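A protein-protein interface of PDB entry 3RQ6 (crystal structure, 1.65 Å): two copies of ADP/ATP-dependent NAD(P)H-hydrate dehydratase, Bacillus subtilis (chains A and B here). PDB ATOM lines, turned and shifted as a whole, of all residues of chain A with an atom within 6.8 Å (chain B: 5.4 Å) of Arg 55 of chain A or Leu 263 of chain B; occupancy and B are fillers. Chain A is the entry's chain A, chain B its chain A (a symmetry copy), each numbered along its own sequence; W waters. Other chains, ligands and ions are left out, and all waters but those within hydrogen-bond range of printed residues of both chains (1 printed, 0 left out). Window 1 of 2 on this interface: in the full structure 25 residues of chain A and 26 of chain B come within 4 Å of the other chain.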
ATOM      1  N   GLY A  50      25.752 -11.423  -3.325  1.00  0.00           N
ATOM      2  CA  GLY A  50      26.122 -10.031  -3.151  1.00  0.00           C
ATOM      3  C   GLY A  50      26.302  -9.633  -1.704  1.00  0.00           C
ATOM      4  O   GLY A  50      27.273  -8.935  -1.332  1.00  0.00           O
ATOM      5  N   LEU A  51      25.349 -10.017  -0.869  1.00  0.00           N
ATOM      6  CA  LEU A  51      25.394  -9.755   0.548  1.00  0.00           C
ATOM      7  C   LEU A  51      26.631 -10.430   1.174  1.00  0.00           C
ATOM      8  O   LEU A  51      27.348  -9.844   1.962  1.00  0.00           O
ATOM      9  CB  LEU A  51      24.141 -10.285   1.207  1.00  0.00           C
ATOM     10  CG  LEU A  51      22.900  -9.475   1.161  1.00  0.00           C
ATOM     11  CD1 LEU A  51      21.669 -10.383   1.514  1.00  0.00           C
ATOM     12  CD2 LEU A  51      23.017  -8.255   2.097  1.00  0.00           C
ATOM     13  N   GLY A  52      26.862 -11.698   0.825  1.00  0.00           N
ATOM     14  CA  GLY A  52      28.026 -12.445   1.334  1.00  0.00           C
ATOM     15  C   GLY A  52      29.301 -11.710   0.974  1.00  0.00           C
ATOM     16  O   GLY A  52      30.181 -11.572   1.777  1.00  0.00           O
ATOM     17  N   ALA A  53      29.381 -11.199  -0.238  1.00  0.00           N
ATOM     18  CA  ALA A  53      30.616 -10.576  -0.713  1.00  0.00           C
ATOM     19  C   ALA A  53      30.848  -9.248  -0.049  1.00  0.00           C
ATOM     20  O   ALA A  53      31.931  -8.971   0.464  1.00  0.00           O
ATOM     21  CB  ALA A  53      30.549 -10.403  -2.235  1.00  0.00           C
ATOM     22  N   MET A  54      29.814  -8.390   0.029  1.00  0.00           N
ATOM     23  CA  MET A  54      29.992  -7.056   0.670  1.00  0.00           C
ATOM     24  C   MET A  54      30.233  -7.136   2.170  1.00  0.00           C
ATOM     25  O   MET A  54      30.889  -6.293   2.737  1.00  0.00           O
ATOM     26  CB  MET A  54      28.852  -6.097   0.292  1.00  0.00           C
ATOM     27  CG  MET A  54      28.790  -5.908  -1.185  1.00  0.00           C
ATOM     28  SD  MET A  54      28.156  -4.275  -1.682  1.00  0.00           S
ATOM     29  CE  MET A  54      29.608  -3.248  -1.380  1.00  0.00           C
ATOM     30  N   ARG A  55      29.669  -8.163   2.793  1.00  0.00           N
ATOM     31  CA  ARG A  55      29.981  -8.442   4.167  1.00  0.00           C
ATOM     32  C   ARG A  55      31.407  -8.884   4.423  1.00  0.00           C
ATOM     33  O   ARG A  55      31.809  -8.884   5.596  1.00  0.00           O
ATOM     34  CB  ARG A  55      29.032  -9.544   4.710  1.00  0.00           C
ATOM     35  CG  ARG A  55      27.639  -9.015   5.049  1.00  0.00           C
ATOM     36  CD  ARG A  55      27.656  -8.217   6.285  1.00  0.00           C
ATOM     37  NE  ARG A  55      26.289  -7.963   6.789  1.00  0.00           N
ATOM     38  CZ  ARG A  55      25.955  -6.929   7.582  1.00  0.00           C
ATOM     39  NH1 ARG A  55      26.819  -5.974   7.908  1.00  0.00           N
ATOM     40  NH2 ARG A  55      24.702  -6.778   7.991  1.00  0.00           N
ATOM     41  N   SER A  56      32.113  -9.331   3.410  1.00  0.00           N
ATOM     42  CA  SER A  56      33.359 -10.045   3.628  1.00  0.00           C
ATOM     43  C   SER A  56      34.604  -9.289   3.236  1.00  0.00           C
ATOM     44  O   SER A  56      35.610  -9.887   2.834  1.00  0.00           O
ATOM     45  CB  SER A  56      33.282 -11.427   2.974  1.00  0.00           C
ATOM     46  OG  SER A  56      32.294 -12.234   3.592  1.00  0.00           O
ATOM     47  N   GLY A  57      34.603  -7.982   3.466  1.00  0.00           N
ATOM     48  CA  GLY A  57      35.833  -7.214   3.470  1.00  0.00           C
ATOM     49  C   GLY A  57      36.362  -6.652   2.146  1.00  0.00           C
ATOM     50  O   GLY A  57      37.477  -6.103   2.160  1.00  0.00           O
ATOM     51  N   LEU A  58      35.578  -6.712   1.064  1.00  0.00           N
ATOM     52  CA  LEU A  58      35.964  -6.044  -0.125  1.00  0.00           C
ATOM     53  C   LEU A  58      35.873  -4.513   0.011  1.00  0.00           C
ATOM     54  O   LEU A  58      35.421  -3.984   1.034  1.00  0.00           O
ATOM     55  CB  LEU A  58      35.170  -6.567  -1.309  1.00  0.00           C
ATOM     56  CG  LEU A  58      33.641  -6.578  -1.197  1.00  0.00           C
ATOM     57  CD1 LEU A  58      32.998  -5.193  -1.102  1.00  0.00           C
ATOM     58  CD2 LEU A  58      32.986  -7.251  -2.374  1.00  0.00           C
ATOM     59  N   VAL A  76      17.966  -3.948  -0.587  1.00  0.00           N
ATOM     60  CA  VAL A  76      18.608  -4.742   0.462  1.00  0.00           C
ATOM     61  C   VAL A  76      20.136  -4.460   0.566  1.00  0.00           C
ATOM     62  O   VAL A  76      20.689  -4.418   1.701  1.00  0.00           O
ATOM     63  CB  VAL A  76      18.331  -6.260   0.270  1.00  0.00           C
ATOM     64  CG1 VAL A  76      18.990  -7.102   1.339  1.00  0.00           C
ATOM     65  CG2 VAL A  76      16.784  -6.556   0.214  1.00  0.00           C
ATOM     66  N   LEU A  77      20.752  -4.194  -0.598  1.00  0.00           N
ATOM     67  CA  LEU A  77      22.209  -4.057  -0.709  1.00  0.00           C
ATOM     68  C   LEU A  77      22.454  -2.822  -1.599  1.00  0.00           C
ATOM     69  O   LEU A  77      22.904  -2.940  -2.774  1.00  0.00           O
ATOM     70  CB  LEU A  77      22.798  -5.332  -1.312  1.00  0.00           C
ATOM     71  CG  LEU A  77      24.317  -5.339  -1.281  1.00  0.00           C
ATOM     72  CD1 LEU A  77      24.946  -5.404   0.159  1.00  0.00           C
ATOM     73  CD2 LEU A  77      24.821  -6.508  -2.166  1.00  0.00           C
ATOM     74  N   GLU A  79      24.642  -0.693  -1.504  1.00  0.00           N
ATOM     75  CA  GLU A  79      26.057  -0.418  -1.668  1.00  0.00           C
ATOM     76  C   GLU A  79      26.708  -0.999  -2.914  1.00  0.00           C
ATOM     77  O   GLU A  79      27.780  -0.533  -3.273  1.00  0.00           O
ATOM     78  CB  GLU A  79      26.828  -0.944  -0.449  1.00  0.00           C
ATOM     79  CG  GLU A  79      26.325  -0.397   0.879  1.00  0.00           C
ATOM     80  CD  GLU A  79      25.033  -1.007   1.481  1.00  0.00           C
ATOM     81  OE1 GLU A  79      24.507  -2.036   0.980  1.00  0.00           O
ATOM     82  OE2 GLU A  79      24.621  -0.429   2.529  1.00  0.00           O
ATOM     83  N   GLY A 223      29.774 -15.719  -2.295  1.00  0.00           N
ATOM     84  CA  GLY A 223      30.035 -14.316  -2.040  1.00  0.00           C
ATOM     85  C   GLY A 223      31.052 -14.078  -0.944  1.00  0.00           C
ATOM     86  O   GLY A 223      31.924 -13.220  -1.076  1.00  0.00           O
ATOM     87  N   MET A 224      30.985 -14.878   0.083  1.00  0.00           N
ATOM     88  CA  MET A 224      31.939 -14.760   1.191  1.00  0.00           C
ATOM     89  C   MET A 224      33.379 -15.021   0.685  1.00  0.00           C
ATOM     90  O   MET A 224      34.314 -14.247   1.016  1.00  0.00           O
ATOM     91  CB  MET A 224      31.562 -15.624   2.377  1.00  0.00           C
ATOM     92  CG  MET A 224      30.354 -15.149   3.092  1.00  0.00           C
ATOM     93  SD  MET A 224      29.922 -16.267   4.470  1.00  0.00           S
ATOM     94  CE  MET A 224      31.445 -16.259   5.463  1.00  0.00           C
ATOM     95  N   GLY A 227      34.468 -11.891  -1.379  1.00  0.00           N
ATOM     96  CA  GLY A 227      34.937 -10.768  -0.575  1.00  0.00           C
ATOM     97  C   GLY A 227      36.253 -11.072   0.147  1.00  0.00           C
ATOM     98  O   GLY A 227      37.189 -10.214   0.163  1.00  0.00           O
ATOM     99  N   MET A 228      36.414 -12.293   0.657  1.00  0.00           N
ATOM    100  CA  MET A 228      37.656 -12.619   1.402  1.00  0.00           C
ATOM    101  C   MET A 228      38.870 -12.641   0.493  1.00  0.00           C
ATOM    102  O   MET A 228      39.929 -12.228   0.905  1.00  0.00           O
ATOM    103  CB  MET A 228      37.484 -13.891   2.242  1.00  0.00           C
ATOM    104  CG  MET A 228      36.611 -13.564   3.516  1.00  0.00           C
ATOM    105  SD  MET A 228      36.625 -14.918   4.645  1.00  0.00           S
ATOM    106  CE  MET A 228      35.168 -14.542   5.580  1.00  0.00           C
ATOM    107  N   LEU A 267      22.997 -15.805   7.403  1.00  0.00           N
ATOM    108  CA  LEU A 267      24.406 -16.046   7.582  1.00  0.00           C
ATOM    109  C   LEU A 267      25.200 -14.737   7.455  1.00  0.00           C
ATOM    110  O   LEU A 267      26.110 -14.498   8.217  1.00  0.00           O
ATOM    111  CB  LEU A 267      24.950 -17.083   6.641  1.00  0.00           C
ATOM    112  CG  LEU A 267      24.433 -18.515   6.819  1.00  0.00           C
ATOM    113  CD1 LEU A 267      24.701 -19.333   5.549  1.00  0.00           C
ATOM    114  CD2 LEU A 267      24.984 -19.204   8.049  1.00  0.00           C
ATOM    115  N   SER A 268      24.853 -13.951   6.487  1.00  0.00           N
ATOM    116  CA  SER A 268      25.463 -12.654   6.273  1.00  0.00           C
ATOM    117  C   SER A 268      25.201 -11.639   7.352  1.00  0.00           C
ATOM    118  O   SER A 268      26.048 -10.757   7.566  1.00  0.00           O
ATOM    119  CB  SER A 268      24.983 -12.063   4.924  1.00  0.00           C
ATOM    120  OG  SER A 268      25.375 -12.855   3.859  1.00  0.00           O
ATOM    121  N   ASP A 269      24.056 -11.731   8.026  1.00  0.00           N
ATOM    122  CA  ASP A 269      23.680 -10.867   9.165  1.00  0.00           C
ATOM    123  C   ASP A 269      24.513 -11.285  10.386  1.00  0.00           C
ATOM    124  O   ASP A 269      24.769 -10.450  11.285  1.00  0.00           O
ATOM    125  CB  ASP A 269      22.205 -11.023   9.652  1.00  0.00           C
ATOM    126  CG  ASP A 269      21.077 -10.648   8.654  1.00  0.00           C
ATOM    127  OD1 ASP A 269      21.274  -9.822   7.772  1.00  0.00           O
ATOM    128  OD2 ASP A 269      19.906 -11.178   8.853  1.00  0.00           O
ATOM    129  N   ILE A 270      24.866 -12.580  10.479  1.00  0.00           N
ATOM    130  CA  ILE A 270      25.579 -13.168  11.641  1.00  0.00           C
ATOM    131  C   ILE A 270      27.077 -12.950  11.561  1.00  0.00           C
ATOM    132  O   ILE A 270      27.758 -12.770  12.595  1.00  0.00           O
ATOM    133  CB  ILE A 270      25.257 -14.732  11.779  1.00  0.00           C
ATOM    134  CG1 ILE A 270      23.797 -14.857  12.218  1.00  0.00           C
ATOM    135  CG2 ILE A 270      26.108 -15.469  12.834  1.00  0.00           C
ATOM    136  CD1 ILE A 270      23.167 -16.259  11.927  1.00  0.00           C
ATOM    137  N   LEU A 271      27.601 -12.973  10.352  1.00  0.00           N
ATOM    138  CA  LEU A 271      29.057 -12.893  10.112  1.00  0.00           C
ATOM    139  C   LEU A 271      29.758 -11.721  10.814  1.00  0.00           C
ATOM    140  O   LEU A 271      30.845 -11.914  11.364  1.00  0.00           O
ATOM    141  CB  LEU A 271      29.326 -12.905   8.601  1.00  0.00           C
ATOM    142  CG  LEU A 271      30.809 -12.863   8.205  1.00  0.00           C
ATOM    143  CD1 LEU A 271      31.545 -14.128   8.627  1.00  0.00           C
ATOM    144  CD2 LEU A 271      30.949 -12.641   6.705  1.00  0.00           C
ATOM    145  N   PRO A 272      29.120 -10.536  10.880  1.00  0.00           N
ATOM    146  CA  PRO A 272      29.840  -9.427  11.583  1.00  0.00           C
ATOM    147  C   PRO A 272      30.258  -9.754  13.006  1.00  0.00           C
ATOM    148  O   PRO A 272      31.365  -9.448  13.420  1.00  0.00           O
ATOM    149  CB  PRO A 272      28.783  -8.335  11.624  1.00  0.00           C
ATOM    150  CG  PRO A 272      28.045  -8.494  10.288  1.00  0.00           C
ATOM    151  CD  PRO A 272      27.925 -10.020  10.165  1.00  0.00           C
ATOM    152  N   TRP A 275      32.865 -12.956  13.006  1.00  0.00           N
ATOM    153  CA  TRP A 275      34.210 -12.566  12.561  1.00  0.00           C
ATOM    154  C   TRP A 275      34.919 -11.834  13.719  1.00  0.00           C
ATOM    155  O   TRP A 275      36.085 -12.075  13.971  1.00  0.00           O
ATOM    156  CB  TRP A 275      34.115 -11.723  11.301  1.00  0.00           C
ATOM    157  CG  TRP A 275      35.392 -11.425  10.515  1.00  0.00           C
ATOM    158  CD1 TRP A 275      36.640 -11.204  10.998  1.00  0.00           C
ATOM    159  CD2 TRP A 275      35.473 -11.265   9.091  1.00  0.00           C
ATOM    160  NE1 TRP A 275      37.495 -10.922   9.979  1.00  0.00           N
ATOM    161  CE2 TRP A 275      36.823 -10.962   8.784  1.00  0.00           C
ATOM    162  CE3 TRP A 275      34.567 -11.364   8.054  1.00  0.00           C
ATOM    163  CZ2 TRP A 275      37.259 -10.716   7.487  1.00  0.00           C
ATOM    164  CZ3 TRP A 275      35.005 -11.141   6.777  1.00  0.00           C
ATOM    165  CH2 TRP A 275      36.351 -10.835   6.495  1.00  0.00           C
ATOM    166  N   LYS B 214      34.643   1.238   2.288  1.00  0.00           N
ATOM    167  CA  LYS B 214      33.814   0.361   1.468  1.00  0.00           C
ATOM    168  C   LYS B 214      32.769   1.188   0.793  1.00  0.00           C
ATOM    169  O   LYS B 214      32.350   2.213   1.332  1.00  0.00           O
ATOM    170  CB  LYS B 214      33.170  -0.705   2.348  1.00  0.00           C
ATOM    171  CG  LYS B 214      32.531  -1.851   1.594  1.00  0.00           C
ATOM    172  CD  LYS B 214      31.845  -2.925   2.490  1.00  0.00           C
ATOM    173  CE  LYS B 214      32.825  -3.655   3.438  1.00  0.00           C
ATOM    174  NZ  LYS B 214      32.032  -4.496   4.408  1.00  0.00           N
ATOM    175  N   TRP B 253      30.104   0.420  15.729  1.00  0.00           N
ATOM    176  CA  TRP B 253      30.045  -0.844  15.055  1.00  0.00           C
ATOM    177  C   TRP B 253      31.178  -1.793  15.392  1.00  0.00           C
ATOM    178  O   TRP B 253      30.942  -2.999  15.648  1.00  0.00           O
ATOM    179  CB  TRP B 253      30.039  -0.619  13.519  1.00  0.00           C
ATOM    180  CG  TRP B 253      30.175  -1.860  12.689  1.00  0.00           C
ATOM    181  CD1 TRP B 253      31.303  -2.398  12.111  1.00  0.00           C
ATOM    182  CD2 TRP B 253      29.092  -2.714  12.296  1.00  0.00           C
ATOM    183  NE1 TRP B 253      30.978  -3.550  11.428  1.00  0.00           N
ATOM    184  CE2 TRP B 253      29.627  -3.745  11.502  1.00  0.00           C
ATOM    185  CE3 TRP B 253      27.708  -2.699  12.556  1.00  0.00           C
ATOM    186  CZ2 TRP B 253      28.826  -4.750  10.939  1.00  0.00           C
ATOM    187  CZ3 TRP B 253      26.925  -3.714  12.047  1.00  0.00           C
ATOM    188  CH2 TRP B 253      27.488  -4.731  11.241  1.00  0.00           C
ATOM    189  N   HIS B 260      35.680  -5.412   8.916  1.00  0.00           N
ATOM    190  CA  HIS B 260      35.534  -5.825   7.508  1.00  0.00           C
ATOM    191  C   HIS B 260      34.114  -5.935   7.026  1.00  0.00           C
ATOM    192  O   HIS B 260      33.881  -6.060   5.822  1.00  0.00           O
ATOM    193  CB  HIS B 260      36.172  -7.207   7.304  1.00  0.00           C
ATOM    194  CG  HIS B 260      37.656  -7.174   7.432  1.00  0.00           C
ATOM    195  ND1 HIS B 260      38.473  -6.500   6.556  1.00  0.00           N
ATOM    196  CD2 HIS B 260      38.466  -7.667   8.391  1.00  0.00           C
ATOM    197  CE1 HIS B 260      39.734  -6.659   6.925  1.00  0.00           C
ATOM    198  NE2 HIS B 260      39.749  -7.303   8.069  1.00  0.00           N
ATOM    199  N   THR B 261      33.133  -5.886   7.918  1.00  0.00           N
ATOM    200  CA  THR B 261      31.807  -6.421   7.661  1.00  0.00           C
ATOM    201  C   THR B 261      30.688  -5.362   7.610  1.00  0.00           C
ATOM    202  O   THR B 261      29.574  -5.710   7.392  1.00  0.00           O
ATOM    203  CB  THR B 261      31.425  -7.499   8.647  1.00  0.00           C
ATOM    204  OG1 THR B 261      31.246  -6.953   9.990  1.00  0.00           O
ATOM    205  CG2 THR B 261      32.508  -8.593   8.716  1.00  0.00           C
ATOM    206  N   LEU B 262      30.975  -4.103   7.871  1.00  0.00           N
ATOM    207  CA  LEU B 262      29.961  -3.047   7.913  1.00  0.00           C
ATOM    208  C   LEU B 262      29.400  -2.829   6.528  1.00  0.00           C
ATOM    209  O   LEU B 262      30.149  -2.757   5.559  1.00  0.00           O
ATOM    210  CB  LEU B 262      30.577  -1.720   8.378  1.00  0.00           C
ATOM    211  CG  LEU B 262      29.645  -0.510   8.471  1.00  0.00           C
ATOM    212  CD1 LEU B 262      28.524  -0.642   9.491  1.00  0.00           C
ATOM    213  CD2 LEU B 262      30.536   0.747   8.729  1.00  0.00           C
ATOM    214  N   LEU B 263      28.093  -2.607   6.476  1.00  0.00           N
ATOM    215  CA  LEU B 263      27.483  -2.133   5.198  1.00  0.00           C
ATOM    216  C   LEU B 263      27.034  -0.684   5.488  1.00  0.00           C
ATOM    217  O   LEU B 263      26.496  -0.384   6.503  1.00  0.00           O
ATOM    218  CB  LEU B 263      26.288  -2.992   4.789  1.00  0.00           C
ATOM    219  CG  LEU B 263      26.582  -4.468   4.580  1.00  0.00           C
ATOM    220  CD1 LEU B 263      25.313  -5.239   4.335  1.00  0.00           C
ATOM    221  CD2 LEU B 263      27.576  -4.631   3.457  1.00  0.00           C
ATOM    222  N   ALA B 264      27.265   0.201   4.525  1.00  0.00           N
ATOM    223  CA  ALA B 264      27.077   1.650   4.717  1.00  0.00           C
ATOM    224  C   ALA B 264      25.712   1.969   5.301  1.00  0.00           C
ATOM    225  O   ALA B 264      25.593   2.890   6.069  1.00  0.00           O
ATOM    226  CB  ALA B 264      27.194   2.388   3.332  1.00  0.00           C
ATOM    227  N   HIS B 265      24.643   1.322   4.796  1.00  0.00           N
ATOM    228  CA  HIS B 265      23.288   1.692   5.273  1.00  0.00           C
ATOM    229  C   HIS B 265      23.151   1.520   6.746  1.00  0.00           C
ATOM    230  O   HIS B 265      22.321   2.164   7.358  1.00  0.00           O
ATOM    231  CB  HIS B 265      22.176   0.980   4.545  1.00  0.00           C
ATOM    232  CG  HIS B 265      22.109  -0.493   4.762  1.00  0.00           C
ATOM    233  ND1 HIS B 265      22.762  -1.391   3.940  1.00  0.00           N
ATOM    234  CD2 HIS B 265      21.439  -1.230   5.679  1.00  0.00           C
ATOM    235  CE1 HIS B 265      22.485  -2.617   4.356  1.00  0.00           C
ATOM    236  NE2 HIS B 265      21.725  -2.548   5.427  1.00  0.00           N
ATOM    237  N   GLU B 266      23.948   0.624   7.301  1.00  0.00           N
ATOM    238  CA  GLU B 266      23.898   0.413   8.721  1.00  0.00           C
ATOM    239  C   GLU B 266      24.349   1.626   9.529  1.00  0.00           C
ATOM    240  O   GLU B 266      23.983   1.757  10.737  1.00  0.00           O
ATOM    241  CB  GLU B 266      24.681  -0.839   9.109  1.00  0.00           C
ATOM    242  CG  GLU B 266      24.031  -2.083   8.586  1.00  0.00           C
ATOM    243  CD  GLU B 266      24.823  -3.336   8.761  1.00  0.00           C
ATOM    244  OE1 GLU B 266      26.030  -3.383   8.451  1.00  0.00           O
ATOM    245  OE2 GLU B 266      24.178  -4.327   9.228  1.00  0.00           O
ATOM    246  N   LEU B 267      25.212   2.464   8.960  1.00  0.00           N
ATOM    247  CA  LEU B 267      25.581   3.694   9.614  1.00  0.00           C
ATOM    248  C   LEU B 267      24.331   4.493  10.011  1.00  0.00           C
ATOM    249  O   LEU B 267      24.275   5.046  11.087  1.00  0.00           O
ATOM    250  CB  LEU B 267      26.507   4.543   8.790  1.00  0.00           C
ATOM    251  CG  LEU B 267      27.907   3.978   8.523  1.00  0.00           C
ATOM    252  CD1 LEU B 267      28.547   4.702   7.331  1.00  0.00           C
ATOM    253  CD2 LEU B 267      28.808   4.007   9.738  1.00  0.00           C
HETATM  254  O   HOH W   1      20.350  -5.246   4.143  1.00  0.00           O
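The backbone carbonyl oxygen of His 260 of chain B sits at hydrogen-bond distance from the backbone NH of Gly 57 of chain A (3.1 Å). N of Ala 264 of chain B is in hydrogen-bond range of OE2 of Glu 79 of chain A (3.4 Å). O of Met 54 of chain A lies within hydrogen-bond range of NZ of Lys 214 of chain B (2.7 Å). The side-chain carboxylate (OE1) of Glu 266 of chain B lies within salt-bridge range of the guanidinium group (NH1) of Arg 55 of chain A (2.8 Å). ND1 of His 265 of chain B lies within hydrogen-bond range of OE2 of Glu 79 of chain A (2.5 Å). The backbone carbonyl oxygen (O) of Thr 261 of chain B lies within hydrogen-bond range of the guanidinium group (NH1) of Arg 55 of chain A (2.8 Å).
N of Leu 263 of chain B sits at hydrogen-bond distance from OE1 of Glu 266 of chain B. The side-chain amino group (NZ) of Lys 214 of chain B is in hydrogen-bond range of the backbone carbonyl oxygen (O) of His 260 of chain B. The side-chain amino group (NZ) of Lys 214 of chain B lies within hydrogen-bond range of the backbone carbonyl oxygen (O) of Leu 262 of chain B, 2.8 Å away. The guanidinium group (NE) of Arg 55 of chain A sits at hydrogen-bond distance from the backbone carbonyl oxygen (O) of Ser 268 of chain A (2.9 Å).
Among the printed residues, merely in contact across the chains: Pro 272 of chain A with Thr 261 of chain B (3.3 Å), Trp 275 of chain A with His 260 of chain B (3.4 Å), Arg 55 of chain A with His 260 of chain B (3.5 Å), Trp 275 of chain A with Thr 261 of chain B (3.5 Å), Leu 58 of chain A with Lys 214 of chain B (3.6 Å), Arg 55 of chain A with Trp 253 of chain B (3.6 Å), Pro 272 of chain A with Trp 253 of chain B (3.7 Å), Arg 55 of chain A with Leu 263 of chain B (3.7 Å), Val 76 of chain A with His 265 of chain B (3.7 Å), Met 54 of chain A with Leu 263 of chain B (3.7 Å) and Glu 79 of chain A with Leu 263 of chain B (3.8 Å).
Arg 55 of chain A touches just these residues of chain B: Trp 253, His 260, Thr 261, Leu 263 and Glu 266. Leu 263 of chain B touches just these residues of chain A: Met 54, Arg 55 and Glu 79. Of the printed residues of chain A, Glu 266 of chain B touches Arg 55 (2.8 Å). Printed residues of chain B within 4 Å of Gly 57 of chain A: His 260. Printed residues of chain A within 4 Å of Thr 261 of chain B: Arg 55 (2.8 Å), Pro 272 (3.3 Å) and Trp 275 (3.5 Å). Printed residues of chain B within 4 Å of Val 76 of chain A: His 265. Ser 56 of chain A touches none of the printed residues of chain B. Gly 52 of chain A touches none of the printed residues of chain B. The nearest residue of chain A that does not touch Leu 263 of chain B is Leu 77 of chain A (4.2 Å). The nearest printed residue of chain B that does not touch Gly 57 of chain A is Lys 214 of chain B (4.4 Å).
Of the 10 printed residues of chain B, 8 touch a printed residue of chain A. Hydrophobic or aromatic side chains of chain B within 4 Å of the printed part of chain A: Trp 253, His 260, Leu 263, Ala 264 and His 265. Of the 23 printed residues of chain A, 8 touch a printed residue of chain B. Hydrophobic or aromatic side chains of chain A within 4 Å of the printed part of chain B: Met 54, Pro 272 and Trp 275. Among the printed residues, 17 pairs touch across the chains.
1 position is printed for both chains. Of the 17 pairs that touch across the chains among the printed residues, none has its exchanged pair printed and touching as well.
Water W1 lies within hydrogen-bond range of the backbone carbonyl oxygen (O) of Val 76 of chain A (2.6 Å) and a ring nitrogen (NE2) of His 265 of chain B (3.3 Å).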
